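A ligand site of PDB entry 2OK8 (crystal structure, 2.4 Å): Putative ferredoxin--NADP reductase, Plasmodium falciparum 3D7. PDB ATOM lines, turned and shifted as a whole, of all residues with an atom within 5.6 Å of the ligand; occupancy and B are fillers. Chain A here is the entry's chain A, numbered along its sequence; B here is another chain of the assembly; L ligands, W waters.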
ATOM      1  N   THR A  53     -19.523   4.378  31.845  1.00  0.00           N
ATOM      2  CA  THR A  53     -19.363   3.619  30.627  1.00  0.00           C
ATOM      3  C   THR A  53     -17.896   3.209  30.482  1.00  0.00           C
ATOM      4  O   THR A  53     -17.006   3.736  31.146  1.00  0.00           O
ATOM      5  CB  THR A  53     -19.782   4.424  29.381  1.00  0.00           C
ATOM      6  OG1 THR A  53     -19.075   5.663  29.378  1.00  0.00           O
ATOM      7  CG2 THR A  53     -21.313   4.699  29.373  1.00  0.00           C
ATOM      8  N   ARG A 101     -16.185   3.072  21.012  1.00  0.00           N
ATOM      9  CA  ARG A 101     -17.613   3.156  21.297  1.00  0.00           C
ATOM     10  C   ARG A 101     -17.844   2.974  22.789  1.00  0.00           C
ATOM     11  O   ARG A 101     -17.206   2.140  23.413  1.00  0.00           O
ATOM     12  CB  ARG A 101     -18.423   2.158  20.459  1.00  0.00           C
ATOM     13  CG  ARG A 101     -18.077   2.136  18.978  1.00  0.00           C
ATOM     14  CD  ARG A 101     -18.345   3.419  18.303  1.00  0.00           C
ATOM     15  NE  ARG A 101     -18.405   3.299  16.852  1.00  0.00           N
ATOM     16  CZ  ARG A 101     -17.507   3.766  15.983  1.00  0.00           C
ATOM     17  NH1 ARG A 101     -16.420   4.403  16.409  1.00  0.00           N
ATOM     18  NH2 ARG A 101     -17.705   3.601  14.689  1.00  0.00           N
ATOM     19  N   LEU A 102     -18.728   3.801  23.347  1.00  0.00           N
ATOM     20  CA  LEU A 102     -19.074   3.760  24.770  1.00  0.00           C
ATOM     21  C   LEU A 102     -20.197   2.746  25.048  1.00  0.00           C
ATOM     22  O   LEU A 102     -21.148   2.640  24.279  1.00  0.00           O
ATOM     23  CB  LEU A 102     -19.492   5.148  25.250  1.00  0.00           C
ATOM     24  CG  LEU A 102     -18.452   6.291  25.182  1.00  0.00           C
ATOM     25  CD1 LEU A 102     -18.977   7.541  25.845  1.00  0.00           C
ATOM     26  CD2 LEU A 102     -17.137   5.890  25.816  1.00  0.00           C
ATOM     27  N   TYR A 103     -20.058   1.996  26.144  1.00  0.00           N
ATOM     28  CA  TYR A 103     -21.066   1.025  26.586  1.00  0.00           C
ATOM     29  C   TYR A 103     -21.230   1.171  28.072  1.00  0.00           C
ATOM     30  O   TYR A 103     -20.253   1.196  28.790  1.00  0.00           O
ATOM     31  CB  TYR A 103     -20.658  -0.413  26.182  1.00  0.00           C
ATOM     32  CG  TYR A 103     -20.585  -0.510  24.674  1.00  0.00           C
ATOM     33  CD1 TYR A 103     -19.368  -0.395  24.003  1.00  0.00           C
ATOM     34  CD2 TYR A 103     -21.752  -0.590  23.918  1.00  0.00           C
ATOM     35  CE1 TYR A 103     -19.301  -0.410  22.614  1.00  0.00           C
ATOM     36  CE2 TYR A 103     -21.681  -0.595  22.526  1.00  0.00           C
ATOM     37  CZ  TYR A 103     -20.460  -0.507  21.881  1.00  0.00           C
ATOM     38  OH  TYR A 103     -20.402  -0.517  20.494  1.00  0.00           O
ATOM     39  N   SER A 104     -22.470   1.316  28.520  1.00  0.00           N
ATOM     40  CA  SER A 104     -22.720   1.322  29.953  1.00  0.00           C
ATOM     41  C   SER A 104     -22.331  -0.003  30.599  1.00  0.00           C
ATOM     42  O   SER A 104     -22.602  -1.094  30.091  1.00  0.00           O
ATOM     43  CB  SER A 104     -24.182   1.642  30.243  1.00  0.00           C
ATOM     44  OG  SER A 104     -24.499   2.932  29.746  1.00  0.00           O
ATOM     45  N   ALA A 117     -23.720  -4.635  27.816  1.00  0.00           N
ATOM     46  CA  ALA A 117     -24.768  -5.135  26.950  1.00  0.00           C
ATOM     47  C   ALA A 117     -24.681  -4.377  25.643  1.00  0.00           C
ATOM     48  O   ALA A 117     -24.821  -3.157  25.626  1.00  0.00           O
ATOM     49  CB  ALA A 117     -26.137  -4.893  27.595  1.00  0.00           C
ATOM     50  N   ILE A 118     -24.470  -5.104  24.553  1.00  0.00           N
ATOM     51  CA  ILE A 118     -24.209  -4.459  23.263  1.00  0.00           C
ATOM     52  C   ILE A 118     -25.192  -4.893  22.189  1.00  0.00           C
ATOM     53  O   ILE A 118     -25.221  -6.070  21.793  1.00  0.00           O
ATOM     54  CB  ILE A 118     -22.745  -4.709  22.777  1.00  0.00           C
ATOM     55  CG1 ILE A 118     -21.748  -4.299  23.864  1.00  0.00           C
ATOM     56  CG2 ILE A 118     -22.481  -3.977  21.414  1.00  0.00           C
ATOM     57  CD1 ILE A 118     -20.282  -4.568  23.529  1.00  0.00           C
ATOM     58  N   LYS A 119     -25.967  -3.932  21.703  1.00  0.00           N
ATOM     59  CA  LYS A 119     -26.848  -4.145  20.565  1.00  0.00           C
ATOM     60  C   LYS A 119     -26.044  -4.221  19.265  1.00  0.00           C
ATOM     61  O   LYS A 119     -25.121  -3.421  19.029  1.00  0.00           O
ATOM     62  CB  LYS A 119     -27.908  -3.055  20.483  1.00  0.00           C
ATOM     63  CG  LYS A 119     -28.782  -3.173  19.269  1.00  0.00           C
ATOM     64  CD  LYS A 119     -29.823  -2.095  19.206  1.00  0.00           C
ATOM     65  CE  LYS A 119     -30.878  -2.449  18.162  1.00  0.00           C
ATOM     66  NZ  LYS A 119     -31.886  -1.367  18.006  1.00  0.00           N
ATOM     67  N   HIS A 121     -26.028  -3.424  15.621  1.00  0.00           N
ATOM     68  CA  HIS A 121     -26.676  -2.588  14.599  1.00  0.00           C
ATOM     69  C   HIS A 121     -26.381  -3.081  13.184  1.00  0.00           C
ATOM     70  O   HIS A 121     -25.227  -3.394  12.846  1.00  0.00           O
ATOM     71  CB  HIS A 121     -26.254  -1.135  14.737  1.00  0.00           C
ATOM     72  CG  HIS A 121     -26.540  -0.544  16.086  1.00  0.00           C
ATOM     73  ND1 HIS A 121     -27.570   0.330  16.308  1.00  0.00           N
ATOM     74  CD2 HIS A 121     -25.934  -0.734  17.284  1.00  0.00           C
ATOM     75  CE1 HIS A 121     -27.583   0.678  17.587  1.00  0.00           C
ATOM     76  NE2 HIS A 121     -26.607   0.038  18.195  1.00  0.00           N
ATOM     77  N   LYS A 122     -27.437  -3.162  12.371  1.00  0.00           N
ATOM     78  CA  LYS A 122     -27.389  -3.657  10.982  1.00  0.00           C
ATOM     79  C   LYS A 122     -28.119  -2.682  10.062  1.00  0.00           C
ATOM     80  O   LYS A 122     -29.002  -1.947  10.505  1.00  0.00           O
ATOM     81  CB  LYS A 122     -28.046  -5.029  10.868  1.00  0.00           C
ATOM     82  CG  LYS A 122     -27.501  -6.070  11.823  1.00  0.00           C
ATOM     83  CD  LYS A 122     -28.513  -7.151  12.155  1.00  0.00           C
ATOM     84  CE  LYS A 122     -28.355  -7.571  13.623  1.00  0.00           C
ATOM     85  NZ  LYS A 122     -28.385  -9.053  13.812  1.00  0.00           N
ATOM     86  N   TYR A 123     -27.750  -2.715   8.788  1.00  0.00           N
ATOM     87  CA  TYR A 123     -28.346  -1.855   7.759  1.00  0.00           C
ATOM     88  C   TYR A 123     -28.103  -2.426   6.353  1.00  0.00           C
ATOM     89  O   TYR A 123     -27.442  -3.450   6.185  1.00  0.00           O
ATOM     90  CB  TYR A 123     -27.776  -0.424   7.858  1.00  0.00           C
ATOM     91  CG  TYR A 123     -26.316  -0.317   7.480  1.00  0.00           C
ATOM     92  CD1 TYR A 123     -25.928   0.074   6.199  1.00  0.00           C
ATOM     93  CD2 TYR A 123     -25.319  -0.609   8.413  1.00  0.00           C
ATOM     94  CE1 TYR A 123     -24.580   0.164   5.850  1.00  0.00           C
ATOM     95  CE2 TYR A 123     -23.978  -0.513   8.075  1.00  0.00           C
ATOM     96  CZ  TYR A 123     -23.612  -0.123   6.799  1.00  0.00           C
ATOM     97  OH  TYR A 123     -22.272  -0.034   6.474  1.00  0.00           O
ATOM     98  N   GLU A 124     -28.658  -1.741   5.345  1.00  0.00           N
ATOM     99  CA  GLU A 124     -28.488  -2.087   3.936  1.00  0.00           C
ATOM    100  C   GLU A 124     -28.010  -0.843   3.184  1.00  0.00           C
ATOM    101  O   GLU A 124     -27.439  -0.948   2.090  1.00  0.00           O
ATOM    102  CB  GLU A 124     -29.822  -2.548   3.326  1.00  0.00           C
ATOM    103  CG  GLU A 124     -30.579  -3.635   4.115  1.00  0.00           C
ATOM    104  CD  GLU A 124     -32.095  -3.538   3.944  1.00  0.00           C
ATOM    105  OE1 GLU A 124     -32.568  -2.819   3.035  1.00  0.00           O
ATOM    106  OE2 GLU A 124     -32.823  -4.179   4.740  1.00  0.00           O
ATOM    107  N   TYR A 135     -23.021  -4.335   8.976  1.00  0.00           N
ATOM    108  CA  TYR A 135     -22.995  -4.022  10.402  1.00  0.00           C
ATOM    109  C   TYR A 135     -22.328  -2.686  10.700  1.00  0.00           C
ATOM    110  O   TYR A 135     -21.513  -2.207   9.910  1.00  0.00           O
ATOM    111  CB  TYR A 135     -22.288  -5.136  11.169  1.00  0.00           C
ATOM    112  CG  TYR A 135     -22.985  -6.478  11.068  1.00  0.00           C
ATOM    113  CD1 TYR A 135     -22.753  -7.344   9.984  1.00  0.00           C
ATOM    114  CD2 TYR A 135     -23.892  -6.867  12.036  1.00  0.00           C
ATOM    115  CE1 TYR A 135     -23.400  -8.566   9.897  1.00  0.00           C
ATOM    116  CE2 TYR A 135     -24.549  -8.086  11.950  1.00  0.00           C
ATOM    117  CZ  TYR A 135     -24.304  -8.927  10.889  1.00  0.00           C
ATOM    118  OH  TYR A 135     -24.963 -10.135  10.833  1.00  0.00           O
ATOM    119  N   GLY A 136     -22.697  -2.067  11.829  1.00  0.00           N
ATOM    120  CA  GLY A 136     -21.979  -0.928  12.371  1.00  0.00           C
ATOM    121  C   GLY A 136     -20.556  -1.346  12.648  1.00  0.00           C
ATOM    122  O   GLY A 136     -20.262  -2.545  12.698  1.00  0.00           O
ATOM    123  N   TYR A 137     -19.664  -0.376  12.811  1.00  0.00           N
ATOM    124  CA  TYR A 137     -18.251  -0.678  12.989  1.00  0.00           C
ATOM    125  C   TYR A 137     -17.964  -1.538  14.225  1.00  0.00           C
ATOM    126  O   TYR A 137     -17.337  -2.591  14.134  1.00  0.00           O
ATOM    127  CB  TYR A 137     -17.421   0.620  12.996  1.00  0.00           C
ATOM    128  CG  TYR A 137     -15.916   0.438  13.095  1.00  0.00           C
ATOM    129  CD1 TYR A 137     -15.203  -0.347  12.188  1.00  0.00           C
ATOM    130  CD2 TYR A 137     -15.205   1.082  14.099  1.00  0.00           C
ATOM    131  CE1 TYR A 137     -13.799  -0.511  12.295  1.00  0.00           C
ATOM    132  CE2 TYR A 137     -13.819   0.948  14.214  1.00  0.00           C
ATOM    133  CZ  TYR A 137     -13.117   0.160  13.320  1.00  0.00           C
ATOM    134  OH  TYR A 137     -11.758   0.052  13.487  1.00  0.00           O
ATOM    135  N   CYS A 138     -18.427  -1.083  15.392  1.00  0.00           N
ATOM    136  CA  CYS A 138     -18.210  -1.867  16.616  1.00  0.00           C
ATOM    137  C   CYS A 138     -19.126  -3.097  16.654  1.00  0.00           C
ATOM    138  O   CYS A 138     -18.696  -4.183  17.047  1.00  0.00           O
ATOM    139  CB  CYS A 138     -18.366  -1.001  17.861  1.00  0.00           C
ATOM    140  SG  CYS A 138     -17.656  -1.752  19.332  1.00  0.00           S
ATOM    141  N   SER A 139     -20.384  -2.926  16.239  1.00  0.00           N
ATOM    142  CA  SER A 139     -21.349  -4.022  16.080  1.00  0.00           C
ATOM    143  C   SER A 139     -20.805  -5.250  15.334  1.00  0.00           C
ATOM    144  O   SER A 139     -20.919  -6.366  15.816  1.00  0.00           O
ATOM    145  CB  SER A 139     -22.623  -3.530  15.396  1.00  0.00           C
ATOM    146  OG  SER A 139     -23.250  -2.512  16.156  1.00  0.00           O
ATOM    147  N   GLY A 140     -20.205  -5.038  14.151  1.00  0.00           N
ATOM    148  CA  GLY A 140     -19.605  -6.124  13.391  1.00  0.00           C
ATOM    149  C   GLY A 140     -18.470  -6.810  14.110  1.00  0.00           C
ATOM    150  O   GLY A 140     -18.277  -8.020  14.007  1.00  0.00           O
ATOM    151  N   THR A 180     -30.980  -0.617  25.373  1.00  0.00           N
ATOM    152  CA  THR A 180     -29.815  -0.908  26.184  1.00  0.00           C
ATOM    153  C   THR A 180     -29.651   0.091  27.304  1.00  0.00           C
ATOM    154  O   THR A 180     -28.760  -0.082  28.140  1.00  0.00           O
ATOM    155  CB  THR A 180     -28.515  -0.934  25.337  1.00  0.00           C
ATOM    156  OG1 THR A 180     -28.457   0.258  24.535  1.00  0.00           O
ATOM    157  CG2 THR A 180     -28.459  -2.189  24.435  1.00  0.00           C
ATOM    158  N   SER A 183     -28.911  -0.857  31.200  1.00  0.00           N
ATOM    159  CA  SER A 183     -27.656  -1.338  31.792  1.00  0.00           C
ATOM    160  C   SER A 183     -27.176  -0.557  33.006  1.00  0.00           C
ATOM    161  O   SER A 183     -26.879  -1.156  34.022  1.00  0.00           O
ATOM    162  CB  SER A 183     -26.530  -1.436  30.759  1.00  0.00           C
ATOM    163  OG  SER A 183     -26.862  -2.350  29.752  1.00  0.00           O
ATOM    164  N   GLU A 314     -28.217  10.402  30.403  1.00  0.00           N
ATOM    165  CA  GLU A 314     -27.214   9.734  29.603  1.00  0.00           C
ATOM    166  C   GLU A 314     -27.892   9.262  28.331  1.00  0.00           C
ATOM    167  O   GLU A 314     -28.498   8.201  28.313  1.00  0.00           O
ATOM    168  CB  GLU A 314     -26.640   8.534  30.367  1.00  0.00           C
ATOM    169  CG  GLU A 314     -25.529   7.761  29.640  1.00  0.00           C
ATOM    170  CD  GLU A 314     -24.141   8.118  30.157  1.00  0.00           C
ATOM    171  OE1 GLU A 314     -23.453   7.199  30.674  1.00  0.00           O
ATOM    172  OE2 GLU A 314     -23.747   9.310  30.067  1.00  0.00           O
ATOM    173  N   VAL A 315     -27.818  10.043  27.263  1.00  0.00           N
ATOM    174  CA  VAL A 315     -28.509   9.688  26.030  1.00  0.00           C
ATOM    175  C   VAL A 315     -27.570   9.536  24.821  1.00  0.00           C
ATOM    176  O   VAL A 315     -26.439  10.012  24.854  1.00  0.00           O
ATOM    177  CB  VAL A 315     -29.725  10.635  25.701  1.00  0.00           C
ATOM    178  CG1 VAL A 315     -30.891  10.366  26.648  1.00  0.00           C
ATOM    179  CG2 VAL A 315     -29.321  12.106  25.734  1.00  0.00           C
ATOM    180  N   TYR A 316     -28.052   8.847  23.796  1.00  0.00           N
ATOM    181  CA  TYR A 316     -27.240   8.507  22.618  1.00  0.00           C
ATOM    182  C   TYR A 316     -28.020   8.038  21.379  1.00  0.00           C
ATOM    183  O   TYR A 316     -29.233   8.251  21.259  1.00  0.00           O
ATOM    184  CB  TYR A 316     -26.215   7.452  22.984  1.00  0.00           C
ATOM    185  CG  TYR A 316     -26.743   6.203  23.695  1.00  0.00           C
ATOM    186  CD1 TYR A 316     -27.131   5.078  22.980  1.00  0.00           C
ATOM    187  CD2 TYR A 316     -26.766   6.137  25.092  1.00  0.00           C
ATOM    188  CE1 TYR A 316     -27.555   3.918  23.637  1.00  0.00           C
ATOM    189  CE2 TYR A 316     -27.193   4.999  25.745  1.00  0.00           C
ATOM    190  CZ  TYR A 316     -27.583   3.896  25.025  1.00  0.00           C
ATOM    191  OH  TYR A 316     -28.005   2.762  25.697  1.00  0.00           O
ATOM    192  N   LYS B  13     -15.650  -0.514   7.683  1.00  0.00           N
ATOM    193  CA  LYS B  13     -16.380  -1.781   7.677  1.00  0.00           C
ATOM    194  C   LYS B  13     -15.627  -2.818   6.861  1.00  0.00           C
ATOM    195  O   LYS B  13     -15.591  -3.986   7.247  1.00  0.00           O
ATOM    196  CB  LYS B  13     -17.802  -1.593   7.128  1.00  0.00           C
ATOM    197  CG  LYS B  13     -18.845  -1.187   8.176  1.00  0.00           C
ATOM    198  CD  LYS B  13     -18.632   0.198   8.745  1.00  0.00           C
ATOM    199  CE  LYS B  13     -19.239   1.276   7.869  1.00  0.00           C
ATOM    200  NZ  LYS B  13     -20.577   1.695   8.371  1.00  0.00           N
HETATM  201  P1  LIG L   1     -21.549   2.908  13.653  1.00  0.00           P
HETATM  202  O1  LIG L   1     -20.854   3.982  14.457  1.00  0.00           O
HETATM  203  O2  LIG L   1     -20.697   2.242  12.614  1.00  0.00           O
HETATM  204  O3  LIG L   1     -22.835   3.590  13.033  1.00  0.00           O
HETATM  205  C1  LIG L   1     -23.774   4.245  13.863  1.00  0.00           C
HETATM  206  C2  LIG L   1     -25.168   3.858  13.387  1.00  0.00           C
HETATM  207  O4  LIG L   1     -25.284   4.216  12.017  1.00  0.00           O
HETATM  208  C3  LIG L   1     -25.373   2.348  13.496  1.00  0.00           C
HETATM  209  O5  LIG L   1     -26.710   2.061  13.866  1.00  0.00           O
HETATM  210  C4  LIG L   1     -25.137   1.838  12.098  1.00  0.00           C
HETATM  211  O6  LIG L   1     -25.852   0.658  11.786  1.00  0.00           O
HETATM  212  C5  LIG L   1     -25.547   3.042  11.253  1.00  0.00           C
HETATM  213  N1  LIG L   1     -24.827   3.071   9.979  1.00  0.00           N
HETATM  214  C6  LIG L   1     -23.470   2.971   9.777  1.00  0.00           C
HETATM  215  N2  LIG L   1     -23.232   3.035   8.447  1.00  0.00           N
HETATM  216  C7  LIG L   1     -24.413   3.176   7.812  1.00  0.00           C
HETATM  217  C8  LIG L   1     -24.746   3.287   6.464  1.00  0.00           C
HETATM  218  N3  LIG L   1     -23.836   3.839   5.668  1.00  0.00           N
HETATM  219  N4  LIG L   1     -26.073   3.402   6.110  1.00  0.00           N
HETATM  220  C9  LIG L   1     -27.075   3.424   7.079  1.00  0.00           C
HETATM  221  N5  LIG L   1     -26.741   3.320   8.414  1.00  0.00           N
HETATM  222  C10 LIG L   1     -25.428   3.198   8.763  1.00  0.00           C
HETATM  223  N6  LIG L   1     -24.805   0.921  22.869  1.00  0.00           N
HETATM  224  C11 LIG L   1     -25.163  -0.303  23.399  1.00  0.00           C
HETATM  225  O7  LIG L   1     -25.455  -1.237  22.660  1.00  0.00           O
HETATM  226  N7  LIG L   1     -25.191  -0.478  24.759  1.00  0.00           N
HETATM  227  C12 LIG L   1     -24.883   0.533  25.624  1.00  0.00           C
HETATM  228  O8  LIG L   1     -24.933   0.300  26.844  1.00  0.00           O
HETATM  229  C13 LIG L   1     -24.515   1.779  25.107  1.00  0.00           C
HETATM  230  N8  LIG L   1     -24.201   2.844  25.936  1.00  0.00           N
HETATM  231  C14 LIG L   1     -23.831   4.066  25.414  1.00  0.00           C
HETATM  232  C15 LIG L   1     -23.524   5.125  26.289  1.00  0.00           C
HETATM  233  C16 LIG L   1     -23.163   6.358  25.756  1.00  0.00           C
HETATM  234  C17 LIG L   1     -22.810   7.485  26.689  1.00  0.00           C
HETATM  235  C18 LIG L   1     -23.098   6.554  24.362  1.00  0.00           C
HETATM  236  C19 LIG L   1     -22.703   7.883  23.788  1.00  0.00           C
HETATM  237  C20 LIG L   1     -23.412   5.500  23.498  1.00  0.00           C
HETATM  238  C21 LIG L   1     -23.782   4.247  24.027  1.00  0.00           C
HETATM  239  N9  LIG L   1     -24.106   3.186  23.199  1.00  0.00           N
HETATM  240  C22 LIG L   1     -24.478   1.955  23.723  1.00  0.00           C
HETATM  241  C23 LIG L   1     -24.057   3.316  21.718  1.00  0.00           C
HETATM  242  C24 LIG L   1     -22.879   2.470  21.224  1.00  0.00           C
HETATM  243  O9  LIG L   1     -21.745   3.285  21.388  1.00  0.00           O
HETATM  244  C25 LIG L   1     -23.133   1.970  19.788  1.00  0.00           C
HETATM  245  O10 LIG L   1     -22.818   0.606  19.441  1.00  0.00           O
HETATM  246  C26 LIG L   1     -22.414   2.855  18.843  1.00  0.00           C
HETATM  247  O11 LIG L   1     -22.715   4.189  19.215  1.00  0.00           O
HETATM  248  C27 LIG L   1     -22.890   2.438  17.450  1.00  0.00           C
HETATM  249  O12 LIG L   1     -22.019   1.374  17.181  1.00  0.00           O
HETATM  250  P2  LIG L   1     -21.386   0.961  15.775  1.00  0.00           P
HETATM  251  O13 LIG L   1     -19.904   1.237  15.785  1.00  0.00           O
HETATM  252  O14 LIG L   1     -21.623  -0.515  15.706  1.00  0.00           O
HETATM  253  O15 LIG L   1     -22.178   1.778  14.633  1.00  0.00           O
HETATM  254  O   HOH W   1     -19.886   6.016  21.179  1.00  0.00           O
HETATM  255  O   HOH W   2     -21.442   5.011  17.003  1.00  0.00           O
HETATM  256  O   HOH W   3     -26.590   1.996  28.010  1.00  0.00           O
HETATM  257  O   HOH W   4     -24.369  -2.029  28.417  1.00  0.00           O
HETATM  258  O   HOH W   5     -26.874   1.290  20.691  1.00  0.00           O
HETATM  259  O   HOH W   6     -24.737  -1.033  20.201  1.00  0.00           O
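O5 of the ligand sits at hydrogen-bond distance from ND1 of His 121 (3.1 Å).
The side-chain hydroxyl (OG1) of Thr 180 sits at hydrogen-bond distance from a nitrogen (N7) of the ligand, 3.4 Å away.
The backbone NH of Ser 104 lies within hydrogen-bond range of an oxygen (O8) of the ligand.
O7 of the ligand sits at hydrogen-bond distance from N of Lys 119.
N7 of the ligand sits at hydrogen-bond distance from O of Ala 117.
OH of Tyr 103 is in hydrogen-bond range of O10 of the ligand, at 2.9 Å.
The side-chain amino group (NZ) of Lys 13 of chain B is in hydrogen-bond range of a nitrogen (N2) of the ligand, at 3.0 Å.
OG of Ser 139 is in hydrogen-bond range of O14 of the ligand (2.6 Å).
The guanidinium group of Arg 101 lies within salt-bridge range of an oxygen (O13) of the ligand, at 2.8 Å.
The backbone NH (N) of Tyr 137 sits at hydrogen-bond distance from an oxygen (O2) of the ligand (2.8 Å).
The backbone NH of Ser 139 is in hydrogen-bond range of an oxygen (O14) of the ligand (2.8 Å).
An oxygen (O13) of the ligand lies within hydrogen-bond range of the backbone NH (N) of Cys 138, 2.8 Å away.
The backbone carbonyl oxygen (O) of Leu 102 is in hydrogen-bond range of an oxygen (O9) of the ligand.
OG1 of Thr 180 is in hydrogen-bond range of OH of Tyr 316.
SG of Cys 138 is in hydrogen-bond range of OH of Tyr 103, at 3.2 Å.
The side-chain amino group (NZ) of Lys 13 of chain B lies within hydrogen-bond range of the side-chain hydroxyl (OH) of Tyr 123 (3.1 Å).
The backbone carbonyl oxygen (O) of Thr 180 sits at hydrogen-bond distance from the side-chain hydroxyl (OG) of Ser 183.
The backbone carbonyl oxygen of His 121 sits at hydrogen-bond distance from the backbone NH of Gly 136 (3.0 Å).
The side-chain hydroxyl (OG) of Ser 139 lies within hydrogen-bond range of the backbone NH (N) of His 121 (3.0 Å).
Thr 53 touches the ligand (CG2 to C15, 3.8 Å).
Ile 118 touches the ligand.
CE1 of Tyr 123 touches C8 of the ligand, at 3.2 Å.
C of Gly 136 touches O14 of the ligand, 3.3 Å away.
Glu 314 touches the ligand (CD to C17, 3.8 Å).
CG of Tyr 316 touches C20 of the ligand (3.4 Å).
Hydrophobic or aromatic side chains within 4 Å of the ligand: Leu 102, Tyr 103, His 121, Tyr 123, Tyr 137 and Tyr 316.
Of the 24 residues printed, 18 come within 4 Å of the ligand.
Water W6 lies within hydrogen-bond range of an oxygen (O7) of the ligand (2.6 Å), the backbone carbonyl oxygen (O) of Lys 119 (2.7 Å) and a ring nitrogen (NE2) of His 121 (2.9 Å).
Water W3 lies within hydrogen-bond range of O8 of the ligand (2.6 Å), OH of Tyr 316 (2.8 Å), OG of Ser 104 (2.9 Å) and O of Thr 180 (3.0 Å).
Water W2 lies within hydrogen-bond range of O11 of the ligand and NE of Arg 101.
Water W4 lies within hydrogen-bond range of O of Ser 104 (2.6 Å), N of Ala 117 (2.8 Å), OG of Ser 183 (2.8 Å) and O8 of the ligand (2.9 Å).
Water W5 lies within hydrogen-bond range of a ring nitrogen (NE2) of His 121 (2.8 Å) and a nitrogen (N6) of the ligand (3.0 Å).
Water W1 lies within hydrogen-bond range of the backbone NH of Leu 102 (3.3 Å) and an oxygen (O9) of the ligand (3.3 Å).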
